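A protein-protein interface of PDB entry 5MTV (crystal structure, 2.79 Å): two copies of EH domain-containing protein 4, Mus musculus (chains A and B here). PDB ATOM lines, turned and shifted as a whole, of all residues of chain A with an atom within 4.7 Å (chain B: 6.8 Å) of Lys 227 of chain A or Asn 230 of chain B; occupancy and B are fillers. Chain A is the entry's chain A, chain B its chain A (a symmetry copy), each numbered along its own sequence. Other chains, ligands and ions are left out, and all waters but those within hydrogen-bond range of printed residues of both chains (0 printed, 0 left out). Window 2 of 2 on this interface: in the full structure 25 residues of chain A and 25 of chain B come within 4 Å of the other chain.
Trp 223 of chain A touches Leu 225 of chain B, and with the chains exchanged Leu 225 of chain A touches Trp 223 of chain B. Trp 223 of chain A touches Gly 226 of chain B, and with the chains exchanged Gly 226 of chain A touches Trp 223 of chain B. Lys 227 of chain A touches Asn 230 of chain B, and with the chains exchanged Asn 230 of chain A touches Lys 227 of chain B. 7 positions are printed for both chains.
NE1 of Trp 223 of chain A lies within hydrogen-bond range of O of Thr 231 of chain B, at 2.9 Å.
Of the 8 printed residues of chain A, 5 touch a printed residue of chain B. Hydrophobic or aromatic side chains of chain A within 4 Å of the printed part of chain B: Trp 223 and Leu 225. Printed residues of chain B that touch a printed residue of chain A: Met 222, Trp 223, Leu 225, Gly 226, Lys 227, Asn 230, Thr 231, Pro 232 and Glu 233. Hydrophobic or aromatic side chains of chain B within 4 Å of the printed part of chain A: Trp 223 and Leu 225.
OD1 of Asn 230 of chain A sits close to O of Lys 227 of chain A, at 3.3 Å. The backbone carbonyl oxygen (O) of Val 228 of chain B sits at hydrogen-bond distance from the side-chain amide nitrogen (ND2) of Asn 230 of chain B, at 3.2 Å. O of Gly 226 of chain B sits close to OD1 of Asn 230 of chain B (3.3 Å). The side-chain amide nitrogen (ND2) of Asn 230 of chain A is in hydrogen-bond range of the backbone carbonyl oxygen (O) of Val 228 of chain A (3.2 Å). The backbone carbonyl oxygen of Lys 227 of chain B lies close to the side-chain amide oxygen of Asn 230 of chain B, at 3.3 Å. O of Gly 226 of chain A sits close to OD1 of Asn 230 of chain A, 3.3 Å away.
Printed residues of chain B within 4 Å of Leu 225 of chain A: Trp 223. Lys 227 of chain A touches just these residues of chain B: Asn 230 (3.7 Å), Thr 231 (3.6 Å) and Pro 232 (3.96 Å). Of the printed residues of chain A, Lys 227 of chain B touches Asn 230 (3.7 Å). Of chain A, only Lys 227 comes within 4 Å of Asn 230 of chain B. Printed residues of chain A within 4 Å of Thr 231 of chain B: Trp 223 (2.9 Å) and Lys 227 (3.6 Å). The nearest residue of chain B that does not touch Lys 227 of chain A is Gly 226 of chain B (4.04 Å). The nearest printed residue of chain A that does not touch Asn 230 of chain B is Trp 223 of chain A (5.1 Å). The nearest printed residue of chain B that does not touch Gly 226 of chain A is Lys 227 of chain B (4.04 Å).
Among the printed residues, merely in contact across the chains: Trp 223 of chain A with Met 222 of chain B (3.4 Å), Trp 223 of chain A with Gly 226 of chain B (3.5 Å), Gly 226 of chain A with Trp 223 of chain B (3.5 Å), Trp 223 of chain A with Glu 233 of chain B (3.6 Å), Trp 223 of chain A with Leu 225 of chain B (3.6 Å), Leu 225 of chain A with Trp 223 of chain B (3.6 Å), Lys 227 of chain A with Thr 231 of chain B (3.6 Å), Asn 230 of chain A with Lys 227 of chain B (3.7 Å), Lys 227 of chain A with Asn 230 of chain B (3.7 Å) and Lys 227 of chain A with Pro 232 of chain B (3.96 Å).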
ATOM      1  N   TRP A 223       2.251 -17.439 -19.701  1.00  0.00           N
ATOM      2  CA  TRP A 223       2.046 -16.090 -19.186  1.00  0.00           C
ATOM      3  C   TRP A 223       1.536 -15.165 -20.281  1.00  0.00           C
ATOM      4  O   TRP A 223       0.501 -14.507 -20.125  1.00  0.00           O
ATOM      5  CB  TRP A 223       3.355 -15.564 -18.595  1.00  0.00           C
ATOM      6  CG  TRP A 223       3.318 -14.131 -18.154  1.00  0.00           C
ATOM      7  CD1 TRP A 223       3.461 -13.025 -18.941  1.00  0.00           C
ATOM      8  CD2 TRP A 223       3.146 -13.649 -16.816  1.00  0.00           C
ATOM      9  NE1 TRP A 223       3.381 -11.886 -18.179  1.00  0.00           N
ATOM     10  CE2 TRP A 223       3.188 -12.242 -16.870  1.00  0.00           C
ATOM     11  CE3 TRP A 223       2.958 -14.271 -15.577  1.00  0.00           C
ATOM     12  CZ2 TRP A 223       3.047 -11.447 -15.736  1.00  0.00           C
ATOM     13  CZ3 TRP A 223       2.819 -13.479 -14.452  1.00  0.00           C
ATOM     14  CH2 TRP A 223       2.864 -12.083 -14.540  1.00  0.00           C
ATOM     15  N   SER A 224       2.250 -15.106 -21.404  1.00  0.00           N
ATOM     16  CA  SER A 224       1.880 -14.214 -22.493  1.00  0.00           C
ATOM     17  C   SER A 224       0.783 -14.781 -23.383  1.00  0.00           C
ATOM     18  O   SER A 224       0.269 -14.052 -24.237  1.00  0.00           O
ATOM     19  CB  SER A 224       3.112 -13.885 -23.341  1.00  0.00           C
ATOM     20  OG  SER A 224       3.743 -15.064 -23.803  1.00  0.00           O
ATOM     21  N   LEU A 225       0.413 -16.051 -23.214  1.00  0.00           N
ATOM     22  CA  LEU A 225      -0.710 -16.598 -23.969  1.00  0.00           C
ATOM     23  C   LEU A 225      -2.037 -16.148 -23.370  1.00  0.00           C
ATOM     24  O   LEU A 225      -2.842 -15.490 -24.038  1.00  0.00           O
ATOM     25  CB  LEU A 225      -0.631 -18.127 -24.011  1.00  0.00           C
ATOM     26  CG  LEU A 225       0.073 -18.753 -25.218  1.00  0.00           C
ATOM     27  CD1 LEU A 225       0.161 -20.261 -25.047  1.00  0.00           C
ATOM     28  CD2 LEU A 225      -0.650 -18.413 -26.516  1.00  0.00           C
ATOM     29  N   GLY A 226      -2.287 -16.504 -22.110  1.00  0.00           N
ATOM     30  CA  GLY A 226      -3.470 -16.001 -21.435  1.00  0.00           C
ATOM     31  C   GLY A 226      -3.568 -14.492 -21.490  1.00  0.00           C
ATOM     32  O   GLY A 226      -4.666 -13.936 -21.561  1.00  0.00           O
ATOM     33  N   LYS A 227      -2.421 -13.808 -21.467  1.00  0.00           N
ATOM     34  CA  LYS A 227      -2.406 -12.357 -21.612  1.00  0.00           C
ATOM     35  C   LYS A 227      -2.969 -11.926 -22.960  1.00  0.00           C
ATOM     36  O   LYS A 227      -3.490 -10.813 -23.090  1.00  0.00           O
ATOM     37  CB  LYS A 227      -0.974 -11.847 -21.440  1.00  0.00           C
ATOM     38  CG  LYS A 227      -0.842 -10.351 -21.238  1.00  0.00           C
ATOM     39  CD  LYS A 227       0.621  -9.959 -21.092  1.00  0.00           C
ATOM     40  CE  LYS A 227       0.789  -8.467 -20.834  1.00  0.00           C
ATOM     41  NZ  LYS A 227       0.283  -7.634 -21.960  1.00  0.00           N
ATOM     42  N   VAL A 228      -2.875 -12.791 -23.970  1.00  0.00           N
ATOM     43  CA  VAL A 228      -3.373 -12.496 -25.310  1.00  0.00           C
ATOM     44  C   VAL A 228      -4.798 -13.011 -25.445  1.00  0.00           C
ATOM     45  O   VAL A 228      -5.735 -12.235 -25.665  1.00  0.00           O
ATOM     46  CB  VAL A 228      -2.458 -13.118 -26.383  1.00  0.00           C
ATOM     47  CG1 VAL A 228      -3.166 -13.208 -27.740  1.00  0.00           C
ATOM     48  CG2 VAL A 228      -1.176 -12.312 -26.512  1.00  0.00           C
ATOM     49  N   ILE A 229      -4.967 -14.328 -25.314  1.00  0.00           N
ATOM     50  CA  ILE A 229      -6.249 -14.950 -25.623  1.00  0.00           C
ATOM     51  C   ILE A 229      -7.334 -14.478 -24.661  1.00  0.00           C
ATOM     52  O   ILE A 229      -8.506 -14.378 -25.044  1.00  0.00           O
ATOM     53  CB  ILE A 229      -6.081 -16.482 -25.631  1.00  0.00           C
ATOM     54  CG1 ILE A 229      -5.055 -16.861 -26.709  1.00  0.00           C
ATOM     55  CG2 ILE A 229      -7.413 -17.180 -25.866  1.00  0.00           C
ATOM     56  CD1 ILE A 229      -4.967 -18.336 -27.039  1.00  0.00           C
ATOM     57  N   ASN A 230      -6.974 -14.164 -23.416  1.00  0.00           N
ATOM     58  CA  ASN A 230      -7.899 -13.538 -22.467  1.00  0.00           C
ATOM     59  C   ASN A 230      -9.148 -14.391 -22.247  1.00  0.00           C
ATOM     60  O   ASN A 230     -10.278 -13.904 -22.321  1.00  0.00           O
ATOM     61  CB  ASN A 230      -8.294 -12.133 -22.933  1.00  0.00           C
ATOM     62  CG  ASN A 230      -7.193 -11.112 -22.727  1.00  0.00           C
ATOM     63  OD1 ASN A 230      -6.448 -11.172 -21.749  1.00  0.00           O
ATOM     64  ND2 ASN A 230      -7.093 -10.161 -23.647  1.00  0.00           N
ATOM     65  N   LYS B 190      -4.182  -8.001  -7.611  1.00  0.00           N
ATOM     66  CA  LYS B 190      -4.385  -6.753  -8.337  1.00  0.00           C
ATOM     67  C   LYS B 190      -4.017  -5.551  -7.475  1.00  0.00           C
ATOM     68  O   LYS B 190      -3.488  -4.554  -7.981  1.00  0.00           O
ATOM     69  CB  LYS B 190      -5.833  -6.654  -8.812  1.00  0.00           C
ATOM     70  CG  LYS B 190      -6.176  -7.605  -9.949  1.00  0.00           C
ATOM     71  CD  LYS B 190      -7.648  -7.524 -10.321  1.00  0.00           C
ATOM     72  CE  LYS B 190      -7.988  -8.461 -11.469  1.00  0.00           C
ATOM     73  NZ  LYS B 190      -9.419  -8.360 -11.870  1.00  0.00           N
ATOM     74  N   ARG B 193      -0.374  -4.682  -7.678  1.00  0.00           N
ATOM     75  CA  ARG B 193       0.157  -4.107  -8.904  1.00  0.00           C
ATOM     76  C   ARG B 193       0.775  -2.744  -8.611  1.00  0.00           C
ATOM     77  O   ARG B 193       0.378  -2.043  -7.677  1.00  0.00           O
ATOM     78  CB  ARG B 193      -0.944  -3.981  -9.957  1.00  0.00           C
ATOM     79  CG  ARG B 193      -0.425  -3.896 -11.384  1.00  0.00           C
ATOM     80  CD  ARG B 193      -1.551  -3.663 -12.380  1.00  0.00           C
ATOM     81  NE  ARG B 193      -2.529  -4.748 -12.378  1.00  0.00           N
ATOM     82  CZ  ARG B 193      -3.638  -4.759 -13.110  1.00  0.00           C
ATOM     83  NH1 ARG B 193      -3.923  -3.738 -13.910  1.00  0.00           N
ATOM     84  NH2 ARG B 193      -4.468  -5.791 -13.044  1.00  0.00           N
ATOM     85  N   MET B 222       0.514 -19.714 -14.463  1.00  0.00           N
ATOM     86  CA  MET B 222       1.070 -18.624 -15.255  1.00  0.00           C
ATOM     87  C   MET B 222       0.050 -18.074 -16.242  1.00  0.00           C
ATOM     88  O   MET B 222       0.055 -16.873 -16.535  1.00  0.00           O
ATOM     89  CB  MET B 222       2.318 -19.105 -15.995  1.00  0.00           C
ATOM     90  CG  MET B 222       3.395 -19.636 -15.072  1.00  0.00           C
ATOM     91  SD  MET B 222       4.089 -18.339 -14.037  1.00  0.00           S
ATOM     92  CE  MET B 222       5.230 -17.570 -15.180  1.00  0.00           C
ATOM     93  N   TRP B 223      -0.827 -18.933 -16.762  1.00  0.00           N
ATOM     94  CA  TRP B 223      -1.873 -18.477 -17.670  1.00  0.00           C
ATOM     95  C   TRP B 223      -2.740 -17.416 -17.006  1.00  0.00           C
ATOM     96  O   TRP B 223      -2.923 -16.319 -17.545  1.00  0.00           O
ATOM     97  CB  TRP B 223      -2.719 -19.671 -18.114  1.00  0.00           C
ATOM     98  CG  TRP B 223      -3.919 -19.321 -18.944  1.00  0.00           C
ATOM     99  CD1 TRP B 223      -5.131 -18.885 -18.492  1.00  0.00           C
ATOM    100  CD2 TRP B 223      -4.028 -19.397 -20.371  1.00  0.00           C
ATOM    101  NE1 TRP B 223      -5.985 -18.678 -19.549  1.00  0.00           N
ATOM    102  CE2 TRP B 223      -5.331 -18.985 -20.713  1.00  0.00           C
ATOM    103  CE3 TRP B 223      -3.149 -19.771 -21.392  1.00  0.00           C
ATOM    104  CZ2 TRP B 223      -5.776 -18.935 -22.031  1.00  0.00           C
ATOM    105  CZ3 TRP B 223      -3.594 -19.721 -22.701  1.00  0.00           C
ATOM    106  CH2 TRP B 223      -4.895 -19.306 -23.007  1.00  0.00           C
ATOM    107  N   LEU B 225      -2.099 -15.836 -14.225  1.00  0.00           N
ATOM    108  CA  LEU B 225      -1.335 -14.770 -13.583  1.00  0.00           C
ATOM    109  C   LEU B 225      -1.133 -13.597 -14.535  1.00  0.00           C
ATOM    110  O   LEU B 225      -1.564 -12.474 -14.255  1.00  0.00           O
ATOM    111  CB  LEU B 225       0.015 -15.302 -13.092  1.00  0.00           C
ATOM    112  CG  LEU B 225       0.083 -15.790 -11.643  1.00  0.00           C
ATOM    113  CD1 LEU B 225       1.453 -16.385 -11.355  1.00  0.00           C
ATOM    114  CD2 LEU B 225      -0.214 -14.659 -10.665  1.00  0.00           C
ATOM    115  N   GLY B 226      -0.468 -13.840 -15.665  1.00  0.00           N
ATOM    116  CA  GLY B 226      -0.353 -12.804 -16.675  1.00  0.00           C
ATOM    117  C   GLY B 226      -1.697 -12.233 -17.073  1.00  0.00           C
ATOM    118  O   GLY B 226      -1.808 -11.044 -17.382  1.00  0.00           O
ATOM    119  N   LYS B 227      -2.738 -13.069 -17.063  1.00  0.00           N
ATOM    120  CA  LYS B 227      -4.089 -12.593 -17.338  1.00  0.00           C
ATOM    121  C   LYS B 227      -4.538 -11.565 -16.307  1.00  0.00           C
ATOM    122  O   LYS B 227      -5.380 -10.711 -16.605  1.00  0.00           O
ATOM    123  CB  LYS B 227      -5.049 -13.784 -17.361  1.00  0.00           C
ATOM    124  CG  LYS B 227      -6.416 -13.500 -17.951  1.00  0.00           C
ATOM    125  CD  LYS B 227      -7.285 -14.748 -17.911  1.00  0.00           C
ATOM    126  CE  LYS B 227      -8.650 -14.513 -18.545  1.00  0.00           C
ATOM    127  NZ  LYS B 227      -9.441 -13.476 -17.825  1.00  0.00           N
ATOM    128  N   VAL B 228      -3.988 -11.629 -15.095  1.00  0.00           N
ATOM    129  CA  VAL B 228      -4.335 -10.705 -14.020  1.00  0.00           C
ATOM    130  C   VAL B 228      -3.366  -9.532 -14.029  1.00  0.00           C
ATOM    131  O   VAL B 228      -3.766  -8.380 -14.229  1.00  0.00           O
ATOM    132  CB  VAL B 228      -4.322 -11.421 -12.656  1.00  0.00           C
ATOM    133  CG1 VAL B 228      -4.246 -10.420 -11.497  1.00  0.00           C
ATOM    134  CG2 VAL B 228      -5.555 -12.299 -12.512  1.00  0.00           C
ATOM    135  N   ILE B 229      -2.083  -9.823 -13.810  1.00  0.00           N
ATOM    136  CA  ILE B 229      -1.104  -8.764 -13.595  1.00  0.00           C
ATOM    137  C   ILE B 229      -0.939  -7.908 -14.847  1.00  0.00           C
ATOM    138  O   ILE B 229      -0.672  -6.704 -14.747  1.00  0.00           O
ATOM    139  CB  ILE B 229       0.223  -9.387 -13.118  1.00  0.00           C
ATOM    140  CG1 ILE B 229      -0.027 -10.127 -11.797  1.00  0.00           C
ATOM    141  CG2 ILE B 229       1.304  -8.326 -12.962  1.00  0.00           C
ATOM    142  CD1 ILE B 229       1.214 -10.569 -11.049  1.00  0.00           C
ATOM    143  N   ASN B 230      -1.112  -8.492 -16.033  1.00  0.00           N
ATOM    144  CA  ASN B 230      -1.149  -7.730 -17.284  1.00  0.00           C
ATOM    145  C   ASN B 230       0.131  -6.922 -17.494  1.00  0.00           C
ATOM    146  O   ASN B 230       0.094  -5.726 -17.787  1.00  0.00           O
ATOM    147  CB  ASN B 230      -2.371  -6.805 -17.325  1.00  0.00           C
ATOM    148  CG  ASN B 230      -3.664  -7.547 -17.592  1.00  0.00           C
ATOM    149  OD1 ASN B 230      -3.693  -8.520 -18.345  1.00  0.00           O
ATOM    150  ND2 ASN B 230      -4.747  -7.082 -16.980  1.00  0.00           N
ATOM    151  N   THR B 231       1.279  -7.586 -17.357  1.00  0.00           N
ATOM    152  CA  THR B 231       2.545  -6.909 -17.591  1.00  0.00           C
ATOM    153  C   THR B 231       3.447  -7.769 -18.466  1.00  0.00           C
ATOM    154  O   THR B 231       3.448  -8.998 -18.331  1.00  0.00           O
ATOM    155  CB  THR B 231       3.267  -6.584 -16.275  1.00  0.00           C
ATOM    156  OG1 THR B 231       3.676  -7.797 -15.629  1.00  0.00           O
ATOM    157  CG2 THR B 231       2.355  -5.805 -15.346  1.00  0.00           C
ATOM    158  N   PRO B 232       4.225  -7.161 -19.368  1.00  0.00           N
ATOM    159  CA  PRO B 232       5.131  -7.968 -20.202  1.00  0.00           C
ATOM    160  C   PRO B 232       6.191  -8.703 -19.403  1.00  0.00           C
ATOM    161  O   PRO B 232       6.649  -9.770 -19.833  1.00  0.00           O
ATOM    162  CB  PRO B 232       5.759  -6.930 -21.146  1.00  0.00           C
ATOM    163  CG  PRO B 232       4.865  -5.744 -21.085  1.00  0.00           C
ATOM    164  CD  PRO B 232       4.291  -5.731 -19.712  1.00  0.00           C
ATOM    165  N   GLU B 233       6.598  -8.165 -18.257  1.00  0.00           N
ATOM    166  CA  GLU B 233       7.645  -8.772 -17.442  1.00  0.00           C
ATOM    167  C   GLU B 233       7.067  -9.984 -16.723  1.00  0.00           C
ATOM    168  O   GLU B 233       6.262  -9.840 -15.797  1.00  0.00           O
ATOM    169  CB  GLU B 233       8.211  -7.757 -16.454  1.00  0.00           C
ATOM    170  CG  GLU B 233       9.029  -6.646 -17.106  1.00  0.00           C
ATOM    171  CD  GLU B 233       8.173  -5.650 -17.865  1.00  0.00           C
ATOM    172  OE1 GLU B 233       7.040  -5.371 -17.416  1.00  0.00           O
ATOM    173  OE2 GLU B 233       8.632  -5.148 -18.914  1.00  0.00           O
